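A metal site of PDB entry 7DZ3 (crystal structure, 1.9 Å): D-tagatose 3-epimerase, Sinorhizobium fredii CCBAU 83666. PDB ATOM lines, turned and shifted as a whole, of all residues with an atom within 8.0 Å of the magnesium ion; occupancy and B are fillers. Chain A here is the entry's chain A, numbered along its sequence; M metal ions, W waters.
NE2 of His 177 sits close to NE2 of His 205, 3.5 Å away. N of His 205 sits at hydrogen-bond distance from O of Leu 178, 2.8 Å away. OE1 of Glu 38 lies within hydrogen-bond range of NE2 of His 205 (2.6 Å). N of Thr 180 sits at hydrogen-bond distance from O of His 205, 3.0 Å away. NH1 of Arg 211 is in salt-bridge range of OD1 of Asp 179 (3.5 Å). The side-chain carboxylate of Glu 240 is in salt-bridge range of the guanidinium group of Arg 211 (3.1 Å). The backbone carbonyl oxygen (O) of Glu 240 lies within hydrogen-bond range of the side-chain hydroxyl (OG) of Ser 207, 3.4 Å away. The backbone NH of Glu 240 sits at hydrogen-bond distance from the backbone carbonyl oxygen of Leu 206 (3.3 Å).
OE1 of Glu 240 touches the magnesium ion, at 3.0 Å. Four residues have an atom within 4 Å of the magnesium ion: Glu 146, Asp 179, His 205 and Glu 240. The nearest printed residue that does not touch the magnesium ion is Arg 211 (4.1 Å).
The magnesium ion is bound by a ring nitrogen (ND1) of His 205, the side-chain carboxylate of Glu 146, the side-chain carboxylate of Asp 179 and water W1. The magnesium ion has four donor atoms within binding distance.
Water W1 lies within hydrogen-bond range of OE2 of Glu 240 and NH2 of Arg 211.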
ATOM      1  N   HIS A   9     -28.391 -33.795  17.000  1.00  0.00           N
ATOM      2  CA  HIS A   9     -26.944 -33.771  16.765  1.00  0.00           C
ATOM      3  C   HIS A   9     -26.449 -35.206  16.870  1.00  0.00           C
ATOM      4  O   HIS A   9     -26.759 -35.900  17.839  1.00  0.00           O
ATOM      5  CB  HIS A   9     -26.308 -32.843  17.780  1.00  0.00           C
ATOM      6  CG  HIS A   9     -24.861 -32.544  17.548  1.00  0.00           C
ATOM      7  ND1 HIS A   9     -23.879 -33.508  17.629  1.00  0.00           N
ATOM      8  CD2 HIS A   9     -24.224 -31.373  17.314  1.00  0.00           C
ATOM      9  CE1 HIS A   9     -22.697 -32.953  17.418  1.00  0.00           C
ATOM     10  NE2 HIS A   9     -22.883 -31.658  17.215  1.00  0.00           N
ATOM     11  N   GLU A  38     -27.894 -33.105  12.520  1.00  0.00           N
ATOM     12  CA  GLU A  38     -26.763 -32.202  12.481  1.00  0.00           C
ATOM     13  C   GLU A  38     -25.497 -33.036  12.493  1.00  0.00           C
ATOM     14  O   GLU A  38     -25.265 -33.813  13.432  1.00  0.00           O
ATOM     15  CB  GLU A  38     -26.782 -31.210  13.639  1.00  0.00           C
ATOM     16  CG  GLU A  38     -25.498 -30.428  13.823  1.00  0.00           C
ATOM     17  CD  GLU A  38     -25.569 -29.464  15.002  1.00  0.00           C
ATOM     18  OE1 GLU A  38     -26.682 -29.231  15.518  1.00  0.00           O
ATOM     19  OE2 GLU A  38     -24.516 -28.931  15.398  1.00  0.00           O
ATOM     20  N   SER A  66     -21.884 -28.872  11.435  1.00  0.00           N
ATOM     21  CA  SER A  66     -21.351 -27.885  12.369  1.00  0.00           C
ATOM     22  C   SER A  66     -19.898 -28.220  12.659  1.00  0.00           C
ATOM     23  O   SER A  66     -19.439 -29.363  12.467  1.00  0.00           O
ATOM     24  CB  SER A  66     -22.128 -27.857  13.695  1.00  0.00           C
ATOM     25  OG  SER A  66     -22.196 -29.163  14.225  1.00  0.00           O
ATOM     26  N   GLY A 103     -22.326 -23.483  14.138  1.00  0.00           N
ATOM     27  CA  GLY A 103     -21.453 -23.782  15.252  1.00  0.00           C
ATOM     28  C   GLY A 103     -20.480 -22.664  15.538  1.00  0.00           C
ATOM     29  O   GLY A 103     -20.752 -21.479  15.284  1.00  0.00           O
ATOM     30  N   VAL A 104     -19.317 -23.046  16.063  1.00  0.00           N
ATOM     31  CA  VAL A 104     -18.283 -22.081  16.436  1.00  0.00           C
ATOM     32  C   VAL A 104     -17.426 -21.844  15.203  1.00  0.00           C
ATOM     33  O   VAL A 104     -16.239 -22.201  15.184  1.00  0.00           O
ATOM     34  CB  VAL A 104     -17.493 -22.548  17.665  1.00  0.00           C
ATOM     35  CG1 VAL A 104     -16.573 -21.453  18.151  1.00  0.00           C
ATOM     36  CG2 VAL A 104     -18.515 -22.952  18.800  1.00  0.00           C
ATOM     37  N   GLU A 146     -22.911 -19.788  16.457  1.00  0.00           N
ATOM     38  CA  GLU A 146     -23.416 -20.311  17.724  1.00  0.00           C
ATOM     39  C   GLU A 146     -22.803 -19.560  18.905  1.00  0.00           C
ATOM     40  O   GLU A 146     -21.584 -19.604  19.100  1.00  0.00           O
ATOM     41  CB  GLU A 146     -23.103 -21.797  17.881  1.00  0.00           C
ATOM     42  CG  GLU A 146     -23.741 -22.400  19.136  1.00  0.00           C
ATOM     43  CD  GLU A 146     -23.397 -23.881  19.383  1.00  0.00           C
ATOM     44  OE1 GLU A 146     -22.497 -24.396  18.704  1.00  0.00           O
ATOM     45  OE2 GLU A 146     -24.071 -24.491  20.245  1.00  0.00           O
ATOM     46  N   ALA A 147     -23.649 -18.966  19.744  1.00  0.00           N
ATOM     47  CA  ALA A 147     -23.178 -18.387  20.992  1.00  0.00           C
ATOM     48  C   ALA A 147     -22.879 -19.503  21.994  1.00  0.00           C
ATOM     49  O   ALA A 147     -23.726 -20.368  22.228  1.00  0.00           O
ATOM     50  CB  ALA A 147     -24.245 -17.442  21.555  1.00  0.00           C
ATOM     51  N   VAL A 148     -21.643 -19.525  22.515  1.00  0.00           N
ATOM     52  CA  VAL A 148     -21.195 -20.513  23.492  1.00  0.00           C
ATOM     53  C   VAL A 148     -20.724 -19.799  24.745  1.00  0.00           C
ATOM     54  O   VAL A 148     -20.458 -18.595  24.754  1.00  0.00           O
ATOM     55  CB  VAL A 148     -20.085 -21.423  22.948  1.00  0.00           C
ATOM     56  CG1 VAL A 148     -20.563 -22.123  21.669  1.00  0.00           C
ATOM     57  CG2 VAL A 148     -18.753 -20.619  22.722  1.00  0.00           C
ATOM     58  N   GLU A 152     -15.683 -21.534  26.985  1.00  0.00           N
ATOM     59  CA  GLU A 152     -15.355 -22.187  25.739  1.00  0.00           C
ATOM     60  C   GLU A 152     -14.742 -21.212  24.757  1.00  0.00           C
ATOM     61  O   GLU A 152     -13.871 -21.579  23.956  1.00  0.00           O
ATOM     62  CB  GLU A 152     -16.602 -22.824  25.158  1.00  0.00           C
ATOM     63  CG  GLU A 152     -17.048 -24.064  25.961  1.00  0.00           C
ATOM     64  CD  GLU A 152     -18.057 -24.922  25.232  1.00  0.00           C
ATOM     65  OE1 GLU A 152     -18.358 -24.625  24.042  1.00  0.00           O
ATOM     66  OE2 GLU A 152     -18.557 -25.857  25.867  1.00  0.00           O
ATOM     67  N   HIS A 177     -27.437 -19.118  16.098  1.00  0.00           N
ATOM     68  CA  HIS A 177     -27.606 -20.481  16.574  1.00  0.00           C
ATOM     69  C   HIS A 177     -27.425 -20.379  18.088  1.00  0.00           C
ATOM     70  O   HIS A 177     -26.362 -19.987  18.578  1.00  0.00           O
ATOM     71  CB  HIS A 177     -26.607 -21.386  15.851  1.00  0.00           C
ATOM     72  CG  HIS A 177     -26.458 -22.754  16.421  1.00  0.00           C
ATOM     73  ND1 HIS A 177     -25.689 -23.720  15.804  1.00  0.00           N
ATOM     74  CD2 HIS A 177     -26.944 -23.331  17.547  1.00  0.00           C
ATOM     75  CE1 HIS A 177     -25.705 -24.824  16.529  1.00  0.00           C
ATOM     76  NE2 HIS A 177     -26.443 -24.605  17.600  1.00  0.00           N
ATOM     77  N   LEU A 178     -28.503 -20.646  18.832  1.00  0.00           N
ATOM     78  CA  LEU A 178     -28.429 -20.633  20.287  1.00  0.00           C
ATOM     79  C   LEU A 178     -28.412 -22.064  20.809  1.00  0.00           C
ATOM     80  O   LEU A 178     -28.772 -23.015  20.121  1.00  0.00           O
ATOM     81  CB  LEU A 178     -29.615 -19.878  20.868  1.00  0.00           C
ATOM     82  CG  LEU A 178     -29.679 -18.385  20.558  1.00  0.00           C
ATOM     83  CD1 LEU A 178     -31.024 -17.784  21.081  1.00  0.00           C
ATOM     84  CD2 LEU A 178     -28.504 -17.696  21.221  1.00  0.00           C
ATOM     85  N   ASP A 179     -28.037 -22.208  22.088  1.00  0.00           N
ATOM     86  CA  ASP A 179     -27.962 -23.511  22.760  1.00  0.00           C
ATOM     87  C   ASP A 179     -28.391 -23.266  24.202  1.00  0.00           C
ATOM     88  O   ASP A 179     -27.793 -22.448  24.896  1.00  0.00           O
ATOM     89  CB  ASP A 179     -26.519 -24.041  22.627  1.00  0.00           C
ATOM     90  CG  ASP A 179     -26.284 -25.358  23.368  1.00  0.00           C
ATOM     91  OD1 ASP A 179     -26.963 -25.636  24.358  1.00  0.00           O
ATOM     92  OD2 ASP A 179     -25.353 -26.101  22.976  1.00  0.00           O
ATOM     93  N   THR A 180     -29.433 -23.975  24.643  1.00  0.00           N
ATOM     94  CA  THR A 180     -29.976 -23.760  25.980  1.00  0.00           C
ATOM     95  C   THR A 180     -28.963 -24.057  27.072  1.00  0.00           C
ATOM     96  O   THR A 180     -29.003 -23.428  28.137  1.00  0.00           O
ATOM     97  CB  THR A 180     -31.231 -24.603  26.166  1.00  0.00           C
ATOM     98  OG1 THR A 180     -30.955 -25.978  25.878  1.00  0.00           O
ATOM     99  CG2 THR A 180     -32.287 -24.159  25.202  1.00  0.00           C
ATOM    100  N   TYR A 181     -28.018 -24.982  26.832  1.00  0.00           N
ATOM    101  CA  TYR A 181     -26.959 -25.214  27.808  1.00  0.00           C
ATOM    102  C   TYR A 181     -26.099 -23.977  27.989  1.00  0.00           C
ATOM    103  O   TYR A 181     -25.726 -23.629  29.110  1.00  0.00           O
ATOM    104  CB  TYR A 181     -26.117 -26.405  27.351  1.00  0.00           C
ATOM    105  CG  TYR A 181     -24.791 -26.597  28.024  1.00  0.00           C
ATOM    106  CD1 TYR A 181     -24.674 -27.328  29.205  1.00  0.00           C
ATOM    107  CD2 TYR A 181     -23.628 -26.096  27.459  1.00  0.00           C
ATOM    108  CE1 TYR A 181     -23.455 -27.550  29.794  1.00  0.00           C
ATOM    109  CE2 TYR A 181     -22.417 -26.317  28.027  1.00  0.00           C
ATOM    110  CZ  TYR A 181     -22.313 -27.024  29.190  1.00  0.00           C
ATOM    111  OH  TYR A 181     -21.056 -27.233  29.729  1.00  0.00           O
ATOM    112  N   HIS A 182     -25.758 -23.302  26.896  1.00  0.00           N
ATOM    113  CA  HIS A 182     -24.934 -22.101  26.985  1.00  0.00           C
ATOM    114  C   HIS A 182     -25.741 -20.941  27.532  1.00  0.00           C
ATOM    115  O   HIS A 182     -25.259 -20.186  28.384  1.00  0.00           O
ATOM    116  CB  HIS A 182     -24.361 -21.783  25.598  1.00  0.00           C
ATOM    117  CG  HIS A 182     -23.376 -22.811  25.115  1.00  0.00           C
ATOM    118  ND1 HIS A 182     -22.286 -23.198  25.867  1.00  0.00           N
ATOM    119  CD2 HIS A 182     -23.302 -23.521  23.960  1.00  0.00           C
ATOM    120  CE1 HIS A 182     -21.588 -24.108  25.205  1.00  0.00           C
ATOM    121  NE2 HIS A 182     -22.178 -24.325  24.048  1.00  0.00           N
ATOM    122  N   TYR A 203     -31.903 -21.574  14.490  1.00  0.00           N
ATOM    123  CA  TYR A 203     -31.514 -22.887  14.960  1.00  0.00           C
ATOM    124  C   TYR A 203     -31.292 -22.836  16.458  1.00  0.00           C
ATOM    125  O   TYR A 203     -30.636 -21.920  16.933  1.00  0.00           O
ATOM    126  CB  TYR A 203     -30.229 -23.327  14.284  1.00  0.00           C
ATOM    127  CG  TYR A 203     -29.940 -24.774  14.352  1.00  0.00           C
ATOM    128  CD1 TYR A 203     -30.672 -25.663  13.606  1.00  0.00           C
ATOM    129  CD2 TYR A 203     -28.873 -25.244  15.075  1.00  0.00           C
ATOM    130  CE1 TYR A 203     -30.365 -27.009  13.620  1.00  0.00           C
ATOM    131  CE2 TYR A 203     -28.571 -26.598  15.110  1.00  0.00           C
ATOM    132  CZ  TYR A 203     -29.326 -27.465  14.381  1.00  0.00           C
ATOM    133  OH  TYR A 203     -29.016 -28.802  14.400  1.00  0.00           O
ATOM    134  N   ILE A 204     -31.770 -23.850  17.196  1.00  0.00           N
ATOM    135  CA  ILE A 204     -31.490 -23.898  18.624  1.00  0.00           C
ATOM    136  C   ILE A 204     -31.171 -25.324  19.060  1.00  0.00           C
ATOM    137  O   ILE A 204     -31.883 -26.263  18.714  1.00  0.00           O
ATOM    138  CB  ILE A 204     -32.675 -23.287  19.429  1.00  0.00           C
ATOM    139  CG1 ILE A 204     -32.278 -23.166  20.910  1.00  0.00           C
ATOM    140  CG2 ILE A 204     -33.899 -24.033  19.250  1.00  0.00           C
ATOM    141  CD1 ILE A 204     -33.219 -22.287  21.721  1.00  0.00           C
ATOM    142  N   HIS A 205     -30.076 -25.486  19.795  1.00  0.00           N
ATOM    143  CA  HIS A 205     -29.772 -26.741  20.460  1.00  0.00           C
ATOM    144  C   HIS A 205     -30.606 -26.805  21.749  1.00  0.00           C
ATOM    145  O   HIS A 205     -30.474 -25.927  22.617  1.00  0.00           O
ATOM    146  CB  HIS A 205     -28.285 -26.868  20.823  1.00  0.00           C
ATOM    147  CG  HIS A 205     -27.410 -27.287  19.676  1.00  0.00           C
ATOM    148  ND1 HIS A 205     -26.054 -27.046  19.645  1.00  0.00           N
ATOM    149  CD2 HIS A 205     -27.705 -27.922  18.503  1.00  0.00           C
ATOM    150  CE1 HIS A 205     -25.543 -27.526  18.520  1.00  0.00           C
ATOM    151  NE2 HIS A 205     -26.521 -28.054  17.803  1.00  0.00           N
ATOM    152  N   LEU A 206     -31.410 -27.849  21.873  1.00  0.00           N
ATOM    153  CA  LEU A 206     -32.153 -28.112  23.110  1.00  0.00           C
ATOM    154  C   LEU A 206     -31.352 -29.125  23.913  1.00  0.00           C
ATOM    155  O   LEU A 206     -31.414 -30.338  23.720  1.00  0.00           O
ATOM    156  CB  LEU A 206     -33.554 -28.616  22.806  1.00  0.00           C
ATOM    157  CG  LEU A 206     -34.327 -27.748  21.833  1.00  0.00           C
ATOM    158  CD1 LEU A 206     -35.549 -28.424  21.341  1.00  0.00           C
ATOM    159  CD2 LEU A 206     -34.696 -26.433  22.473  1.00  0.00           C
ATOM    160  N   SER A 207     -30.530 -28.596  24.800  1.00  0.00           N
ATOM    161  CA  SER A 207     -29.581 -29.360  25.587  1.00  0.00           C
ATOM    162  C   SER A 207     -29.802 -29.064  27.052  1.00  0.00           C
ATOM    163  O   SER A 207     -30.007 -27.916  27.430  1.00  0.00           O
ATOM    164  CB  SER A 207     -28.140 -28.985  25.176  1.00  0.00           C
ATOM    165  OG  SER A 207     -27.191 -29.704  25.942  1.00  0.00           O
ATOM    166  N   ARG A 211     -25.676 -31.217  29.957  1.00  0.00           N
ATOM    167  CA  ARG A 211     -25.541 -31.991  28.728  1.00  0.00           C
ATOM    168  C   ARG A 211     -26.156 -33.375  28.837  1.00  0.00           C
ATOM    169  O   ARG A 211     -25.912 -34.221  27.997  1.00  0.00           O
ATOM    170  CB  ARG A 211     -24.081 -32.084  28.296  1.00  0.00           C
ATOM    171  CG  ARG A 211     -23.457 -30.722  27.938  1.00  0.00           C
ATOM    172  CD  ARG A 211     -24.185 -30.051  26.772  1.00  0.00           C
ATOM    173  NE  ARG A 211     -23.341 -29.072  26.063  1.00  0.00           N
ATOM    174  CZ  ARG A 211     -23.766 -28.358  25.021  1.00  0.00           C
ATOM    175  NH1 ARG A 211     -25.004 -28.508  24.569  1.00  0.00           N
ATOM    176  NH2 ARG A 211     -22.928 -27.508  24.416  1.00  0.00           N
ATOM    177  N   ALA A 238     -33.058 -28.816  17.665  1.00  0.00           N
ATOM    178  CA  ALA A 238     -32.082 -29.898  17.588  1.00  0.00           C
ATOM    179  C   ALA A 238     -31.752 -30.356  18.997  1.00  0.00           C
ATOM    180  O   ALA A 238     -31.228 -29.585  19.812  1.00  0.00           O
ATOM    181  CB  ALA A 238     -30.814 -29.437  16.846  1.00  0.00           C
ATOM    182  N   GLU A 240     -29.533 -32.126  21.635  1.00  0.00           N
ATOM    183  CA  GLU A 240     -28.114 -32.452  21.787  1.00  0.00           C
ATOM    184  C   GLU A 240     -27.838 -32.970  23.187  1.00  0.00           C
ATOM    185  O   GLU A 240     -28.257 -32.364  24.183  1.00  0.00           O
ATOM    186  CB  GLU A 240     -27.229 -31.241  21.478  1.00  0.00           C
ATOM    187  CG  GLU A 240     -25.747 -31.504  21.602  1.00  0.00           C
ATOM    188  CD  GLU A 240     -24.923 -30.270  21.263  1.00  0.00           C
ATOM    189  OE1 GLU A 240     -25.388 -29.161  21.578  1.00  0.00           O
ATOM    190  OE2 GLU A 240     -23.824 -30.402  20.689  1.00  0.00           O
ATOM    191  N   PHE A 242     -24.414 -35.109  25.292  1.00  0.00           N
ATOM    192  CA  PHE A 242     -23.049 -35.614  25.205  1.00  0.00           C
ATOM    193  C   PHE A 242     -22.939 -37.096  25.580  1.00  0.00           C
ATOM    194  O   PHE A 242     -21.824 -37.614  25.607  1.00  0.00           O
ATOM    195  CB  PHE A 242     -22.153 -34.770  26.108  1.00  0.00           C
ATOM    196  CG  PHE A 242     -21.816 -33.395  25.524  1.00  0.00           C
ATOM    197  CD1 PHE A 242     -22.402 -32.944  24.340  1.00  0.00           C
ATOM    198  CD2 PHE A 242     -20.914 -32.568  26.170  1.00  0.00           C
ATOM    199  CE1 PHE A 242     -22.076 -31.694  23.808  1.00  0.00           C
ATOM    200  CE2 PHE A 242     -20.598 -31.316  25.641  1.00  0.00           C
ATOM    201  CZ  PHE A 242     -21.186 -30.887  24.457  1.00  0.00           C
ATOM    202  N   LEU A 253     -14.479 -31.053  25.769  1.00  0.00           N
ATOM    203  CA  LEU A 253     -15.618 -30.212  26.163  1.00  0.00           C
ATOM    204  C   LEU A 253     -15.891 -30.274  27.664  1.00  0.00           C
ATOM    205  O   LEU A 253     -17.000 -29.930  28.113  1.00  0.00           O
ATOM    206  CB  LEU A 253     -16.865 -30.629  25.388  1.00  0.00           C
ATOM    207  CG  LEU A 253     -17.015 -30.148  23.935  1.00  0.00           C
ATOM    208  CD1 LEU A 253     -17.616 -31.314  23.129  1.00  0.00           C
ATOM    209  CD2 LEU A 253     -17.862 -28.883  23.835  1.00  0.00           C
HETATM  210 MG    MG M   1     -24.628 -26.344  20.862  1.00  0.00          MG
HETATM  211  O   HOH W   1     -22.932 -27.811  21.291  1.00  0.00           O
